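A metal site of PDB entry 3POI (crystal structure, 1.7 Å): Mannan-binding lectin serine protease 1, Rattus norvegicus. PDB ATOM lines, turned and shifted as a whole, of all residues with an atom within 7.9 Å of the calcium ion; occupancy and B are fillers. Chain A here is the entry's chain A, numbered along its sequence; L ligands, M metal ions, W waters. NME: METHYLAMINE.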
ATOM      1  N   TYR A  25       8.562 -27.831  15.144  1.00  0.00           N
ATOM      2  CA  TYR A  25       8.256 -29.269  15.369  1.00  0.00           C
ATOM      3  C   TYR A  25       8.174 -30.031  14.059  1.00  0.00           C
ATOM      4  O   TYR A  25       7.887 -29.468  13.006  1.00  0.00           O
ATOM      5  CB  TYR A  25       6.973 -29.422  16.163  1.00  0.00           C
ATOM      6  CG  TYR A  25       5.780 -28.619  15.637  1.00  0.00           C
ATOM      7  CD1 TYR A  25       4.992 -29.060  14.576  1.00  0.00           C
ATOM      8  CD2 TYR A  25       5.396 -27.445  16.253  1.00  0.00           C
ATOM      9  CE1 TYR A  25       3.883 -28.343  14.165  1.00  0.00           C
ATOM     10  CE2 TYR A  25       4.258 -26.740  15.903  1.00  0.00           C
ATOM     11  CZ  TYR A  25       3.518 -27.154  14.820  1.00  0.00           C
ATOM     12  OH  TYR A  25       2.411 -26.446  14.432  1.00  0.00           O
ATOM     13  N   PRO A  26       8.415 -31.348  14.104  1.00  0.00           N
ATOM     14  CA  PRO A  26       8.428 -32.155  12.880  1.00  0.00           C
ATOM     15  C   PRO A  26       7.059 -32.225  12.239  1.00  0.00           C
ATOM     16  O   PRO A  26       6.010 -32.218  12.900  1.00  0.00           O
ATOM     17  CB  PRO A  26       8.825 -33.557  13.415  1.00  0.00           C
ATOM     18  CG  PRO A  26       9.521 -33.324  14.676  1.00  0.00           C
ATOM     19  CD  PRO A  26       8.840 -32.140  15.264  1.00  0.00           C
ATOM     20  N   LYS A  27       7.086 -32.430  10.931  1.00  0.00           N
ATOM     21  CA  LYS A  27       5.842 -32.792  10.248  1.00  0.00           C
ATOM     22  C   LYS A  27       5.325 -34.147  10.687  1.00  0.00           C
ATOM     23  O   LYS A  27       6.092 -35.018  11.087  1.00  0.00           O
ATOM     24  CB  LYS A  27       6.059 -32.736   8.784  1.00  0.00           C
ATOM     25  CG  LYS A  27       6.846 -33.734   8.246  1.00  0.00           C
ATOM     26  CD  LYS A  27       7.007 -33.429   6.682  1.00  0.00           C
ATOM     27  CE  LYS A  27       7.897 -32.288   6.407  1.00  0.00           C
ATOM     28  NZ  LYS A  27       9.238 -32.602   7.085  1.00  0.00           N
ATOM     29  N   SER A  28       4.028 -34.322  10.644  1.00  0.00           N
ATOM     30  CA  SER A  28       3.386 -35.621  10.904  1.00  0.00           C
ATOM     31  C   SER A  28       3.720 -36.157  12.296  1.00  0.00           C
ATOM     32  O   SER A  28       3.805 -37.391  12.500  1.00  0.00           O
ATOM     33  CB  SER A  28       3.744 -36.586   9.777  1.00  0.00           C
ATOM     34  OG  SER A  28       3.229 -36.078   8.563  1.00  0.00           O
ATOM     35  N   ILE A  53       1.382 -22.708  17.161  1.00  0.00           N
ATOM     36  CA  ILE A  53       0.927 -23.903  16.490  1.00  0.00           C
ATOM     37  C   ILE A  53       0.171 -23.444  15.241  1.00  0.00           C
ATOM     38  O   ILE A  53      -0.591 -22.448  15.302  1.00  0.00           O
ATOM     39  CB  ILE A  53       0.030 -24.761  17.414  1.00  0.00           C
ATOM     40  CG1 ILE A  53       0.802 -25.264  18.662  1.00  0.00           C
ATOM     41  CG2 ILE A  53      -0.548 -25.961  16.641  1.00  0.00           C
ATOM     42  CD1 ILE A  53      -0.045 -26.051  19.634  1.00  0.00           C
ATOM     43  N   GLU A  54       0.380 -24.070  14.099  1.00  0.00           N
ATOM     44  CA  GLU A  54      -0.334 -23.659  12.875  1.00  0.00           C
ATOM     45  C   GLU A  54      -1.815 -23.611  13.070  1.00  0.00           C
ATOM     46  O   GLU A  54      -2.387 -24.429  13.778  1.00  0.00           O
ATOM     47  CB  GLU A  54      -0.024 -24.643  11.778  1.00  0.00           C
ATOM     48  CG  GLU A  54      -0.412 -24.161  10.336  1.00  0.00           C
ATOM     49  CD  GLU A  54      -0.127 -25.219   9.275  1.00  0.00           C
ATOM     50  OE1 GLU A  54       0.293 -26.357   9.579  1.00  0.00           O
ATOM     51  OE2 GLU A  54      -0.350 -24.848   8.089  1.00  0.00           O
ATOM     52  N   ASP A  55      -2.431 -22.578  12.521  1.00  0.00           N
ATOM     53  CA  ASP A  55      -3.891 -22.409  12.588  1.00  0.00           C
ATOM     54  C   ASP A  55      -4.505 -22.105  11.211  1.00  0.00           C
ATOM     55  O   ASP A  55      -3.826 -22.201  10.177  1.00  0.00           O
ATOM     56  CB  ASP A  55      -4.268 -21.414  13.658  1.00  0.00           C
ATOM     57  CG  ASP A  55      -3.887 -19.983  13.325  1.00  0.00           C
ATOM     58  OD1 ASP A  55      -4.217 -19.088  14.145  1.00  0.00           O
ATOM     59  OD2 ASP A  55      -3.274 -19.704  12.310  1.00  0.00           O
ATOM     60  N   TYR A  63      -5.152 -28.413  11.379  1.00  0.00           N
ATOM     61  CA  TYR A  63      -3.881 -28.910  10.932  1.00  0.00           C
ATOM     62  C   TYR A  63      -3.088 -29.565  12.057  1.00  0.00           C
ATOM     63  O   TYR A  63      -2.750 -30.745  12.003  1.00  0.00           O
ATOM     64  CB  TYR A  63      -3.090 -27.760  10.320  1.00  0.00           C
ATOM     65  CG  TYR A  63      -3.735 -27.064   9.140  1.00  0.00           C
ATOM     66  CD1 TYR A  63      -4.289 -27.786   8.107  1.00  0.00           C
ATOM     67  CD2 TYR A  63      -3.815 -25.673   9.091  1.00  0.00           C
ATOM     68  CE1 TYR A  63      -4.876 -27.128   6.998  1.00  0.00           C
ATOM     69  CE2 TYR A  63      -4.393 -25.019   7.984  1.00  0.00           C
ATOM     70  CZ  TYR A  63      -4.899 -25.760   6.947  1.00  0.00           C
ATOM     71  OH  TYR A  63      -5.446 -25.110   5.839  1.00  0.00           O
ATOM     72  N   ASP A  64      -2.744 -28.737  13.037  1.00  0.00           N
ATOM     73  CA  ASP A  64      -1.910 -29.120  14.165  1.00  0.00           C
ATOM     74  C   ASP A  64      -2.599 -28.633  15.451  1.00  0.00           C
ATOM     75  O   ASP A  64      -3.277 -27.600  15.445  1.00  0.00           O
ATOM     76  CB  ASP A  64      -0.542 -28.425  14.113  1.00  0.00           C
ATOM     77  CG  ASP A  64       0.192 -28.481  12.740  1.00  0.00           C
ATOM     78  OD1 ASP A  64      -0.122 -29.260  11.864  1.00  0.00           O
ATOM     79  OD2 ASP A  64       1.131 -27.657  12.576  1.00  0.00           O
ATOM     80  N   TYR A  65      -2.426 -29.349  16.551  1.00  0.00           N
ATOM     81  CA  TYR A  65      -2.986 -28.920  17.843  1.00  0.00           C
ATOM     82  C   TYR A  65      -2.498 -29.759  18.983  1.00  0.00           C
ATOM     83  O   TYR A  65      -2.024 -30.879  18.812  1.00  0.00           O
ATOM     84  CB  TYR A  65      -4.530 -28.968  17.802  1.00  0.00           C
ATOM     85  CG  TYR A  65      -5.139 -30.278  17.334  1.00  0.00           C
ATOM     86  CD1 TYR A  65      -5.252 -31.367  18.162  1.00  0.00           C
ATOM     87  CD2 TYR A  65      -5.654 -30.362  16.061  1.00  0.00           C
ATOM     88  CE1 TYR A  65      -5.870 -32.559  17.691  1.00  0.00           C
ATOM     89  CE2 TYR A  65      -6.220 -31.544  15.570  1.00  0.00           C
ATOM     90  CZ  TYR A  65      -6.353 -32.625  16.408  1.00  0.00           C
ATOM     91  OH  TYR A  65      -6.931 -33.780  15.920  1.00  0.00           O
ATOM     92  N   PHE A  98      -0.378 -34.224  21.154  1.00  0.00           N
ATOM     93  CA  PHE A  98      -0.026 -33.229  20.162  1.00  0.00           C
ATOM     94  C   PHE A  98       0.057 -33.926  18.813  1.00  0.00           C
ATOM     95  O   PHE A  98       0.727 -34.978  18.668  1.00  0.00           O
ATOM     96  CB  PHE A  98       1.318 -32.571  20.511  1.00  0.00           C
ATOM     97  CG  PHE A  98       1.832 -31.646  19.403  1.00  0.00           C
ATOM     98  CD1 PHE A  98       1.184 -30.488  19.076  1.00  0.00           C
ATOM     99  CD2 PHE A  98       2.988 -31.930  18.760  1.00  0.00           C
ATOM    100  CE1 PHE A  98       1.666 -29.649  18.061  1.00  0.00           C
ATOM    101  CE2 PHE A  98       3.494 -31.100  17.764  1.00  0.00           C
ATOM    102  CZ  PHE A  98       2.839 -29.985  17.396  1.00  0.00           C
ATOM    103  N   ARG A  99      -0.570 -33.314  17.801  1.00  0.00           N
ATOM    104  CA  ARG A  99      -0.472 -33.819  16.427  1.00  0.00           C
ATOM    105  C   ARG A  99      -0.103 -32.686  15.507  1.00  0.00           C
ATOM    106  O   ARG A  99      -0.567 -31.540  15.678  1.00  0.00           O
ATOM    107  CB  ARG A  99      -1.769 -34.526  15.975  1.00  0.00           C
ATOM    108  CG  ARG A  99      -2.909 -33.631  15.777  1.00  0.00           C
ATOM    109  CD  ARG A  99      -3.172 -33.296  14.304  1.00  0.00           C
ATOM    110  NE  ARG A  99      -3.737 -34.402  13.592  1.00  0.00           N
ATOM    111  CZ  ARG A  99      -4.062 -34.370  12.310  1.00  0.00           C
ATOM    112  NH1 ARG A  99      -4.584 -35.448  11.704  1.00  0.00           N
ATOM    113  NH2 ARG A  99      -3.831 -33.297  11.563  1.00  0.00           N
ATOM    114  N   SER A 100       0.598 -33.049  14.439  1.00  0.00           N
ATOM    115  CA  SER A 100       0.873 -32.106  13.356  1.00  0.00           C
ATOM    116  C   SER A 100       0.674 -32.784  12.025  1.00  0.00           C
ATOM    117  O   SER A 100       0.892 -33.993  11.864  1.00  0.00           O
ATOM    118  CB  SER A 100       2.257 -31.464  13.440  1.00  0.00           C
ATOM    119  OG  SER A 100       3.277 -32.432  13.246  1.00  0.00           O
ATOM    120  N   ASP A 101       0.348 -31.948  11.047  1.00  0.00           N
ATOM    121  CA  ASP A 101       0.185 -32.374   9.654  1.00  0.00           C
ATOM    122  C   ASP A 101       1.464 -32.274   8.885  1.00  0.00           C
ATOM    123  O   ASP A 101       2.552 -32.162   9.478  1.00  0.00           O
ATOM    124  CB  ASP A 101      -0.969 -31.625   9.002  1.00  0.00           C
ATOM    125  CG  ASP A 101      -0.629 -30.193   8.604  1.00  0.00           C
ATOM    126  OD1 ASP A 101       0.504 -29.726   8.927  1.00  0.00           O
ATOM    127  OD2 ASP A 101      -1.484 -29.560   7.930  1.00  0.00           O
ATOM    128  N   ASN A 102       1.396 -32.418   7.562  1.00  0.00           N
ATOM    129  CA  ASN A 102       2.619 -32.653   6.799  1.00  0.00           C
ATOM    130  C   ASN A 102       3.239 -31.390   6.220  1.00  0.00           C
ATOM    131  O   ASN A 102       4.170 -31.510   5.393  1.00  0.00           O
ATOM    132  CB  ASN A 102       2.405 -33.743   5.704  1.00  0.00           C
ATOM    133  CG  ASN A 102       3.698 -34.522   5.353  1.00  0.00           C
ATOM    134  OD1 ASN A 102       4.064 -34.663   4.162  1.00  0.00           O
ATOM    135  ND2 ASN A 102       4.434 -35.010   6.391  1.00  0.00           N
ATOM    136  N   SER A 103       2.849 -30.221   6.698  1.00  0.00           N
ATOM    137  CA  SER A 103       3.471 -29.036   6.226  1.00  0.00           C
ATOM    138  C   SER A 103       3.417 -27.893   7.231  1.00  0.00           C
ATOM    139  O   SER A 103       2.702 -27.927   8.202  1.00  0.00           O
ATOM    140  CB  SER A 103       2.829 -28.614   4.936  1.00  0.00           C
ATOM    141  OG  SER A 103       1.505 -28.317   5.063  1.00  0.00           O
ATOM    142  N   GLY A 104       4.171 -26.866   6.924  1.00  0.00           N
ATOM    143  CA  GLY A 104       4.133 -25.638   7.709  1.00  0.00           C
ATOM    144  C   GLY A 104       5.372 -25.564   8.600  1.00  0.00           C
ATOM    145  O   GLY A 104       6.182 -26.489   8.702  1.00  0.00           O
ATOM    146  N   GLU A 105       5.516 -24.407   9.223  1.00  0.00           N
ATOM    147  CA  GLU A 105       6.652 -24.117  10.072  1.00  0.00           C
ATOM    148  C   GLU A 105       6.202 -23.298  11.263  1.00  0.00           C
ATOM    149  O   GLU A 105       5.826 -22.148  11.082  1.00  0.00           O
ATOM    150  CB  GLU A 105       7.679 -23.333   9.329  1.00  0.00           C
ATOM    151  CG  GLU A 105       8.893 -23.066  10.129  1.00  0.00           C
ATOM    152  CD  GLU A 105       9.918 -22.137   9.397  1.00  0.00           C
ATOM    153  OE1 GLU A 105      10.749 -22.787   8.683  1.00  0.00           O
ATOM    154  OE2 GLU A 105       9.950 -20.813   9.626  1.00  0.00           O
ATOM    155  N   ASN A 106       6.236 -23.891  12.466  1.00  0.00           N
ATOM    156  CA  ASN A 106       5.713 -23.242  13.685  1.00  0.00           C
ATOM    157  C   ASN A 106       6.573 -23.756  14.856  1.00  0.00           C
ATOM    158  O   ASN A 106       6.978 -24.932  14.857  1.00  0.00           O
ATOM    159  CB  ASN A 106       4.228 -23.617  13.894  1.00  0.00           C
ATOM    160  CG  ASN A 106       3.323 -23.033  12.803  1.00  0.00           C
ATOM    161  OD1 ASN A 106       2.838 -21.818  12.893  1.00  0.00           O
ATOM    162  ND2 ASN A 106       3.099 -23.800  11.784  1.00  0.00           N
HETATM  163  N   NME L   1      -0.629 -27.257   6.780  1.00  0.00           N
HETATM  164  C   NME L   1      -1.564 -27.055   5.739  1.00  0.00           C
HETATM  165 CA    CA M   1       1.610 -28.058  10.235  1.00  0.00          CA
HETATM  166  O   HOH W   1       3.403 -26.515  11.025  1.00  0.00           O
HETATM  167  O   HOH W   2       3.175 -29.736  10.749  1.00  0.00           O
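The side-chain carboxylate of Asp 101 is in salt-bridge range of a nitrogen (N) of the ligand (2.7 Å). N of the ligand lies within salt-bridge range of OE2 of Glu 54 (2.8 Å). A nitrogen (N) of the ligand lies within hydrogen-bond range of the side-chain hydroxyl (OG) of Ser 103, 2.9 Å away.
N of Asp 101 sits at hydrogen-bond distance from O of Tyr 63 (3.5 Å). The backbone carbonyl oxygen of Asp 101 sits at hydrogen-bond distance from the backbone NH of Ser 28 (2.9 Å). The side-chain carboxylate (OD2) of Asp 64 sits close to the side-chain hydroxyl (OH) of Tyr 25, at 2.6 Å. The backbone NH (N) of Glu 54 is in hydrogen-bond range of the side-chain hydroxyl (OH) of Tyr 25, at 3.1 Å.
Of the 19 residues printed, 4 come within 4 Å of the calcium ion.
The calcium ion is bound by the side-chain carboxylate (OE1) of Glu 54, the backbone carbonyl oxygen (O) of Ser 103, water W2, the side-chain carboxylate (OD1) of Asp 101, the side-chain carboxylate (OD2) of Asp 64, water W1 and the side-chain carboxylate (OD1) of Asp 64. The calcium ion has seven donor atoms within binding distance.
Water W1 lies within hydrogen-bond range of the side-chain amide nitrogen of Asn 106 (2.8 Å) and the backbone NH of Glu 105 (3.5 Å).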
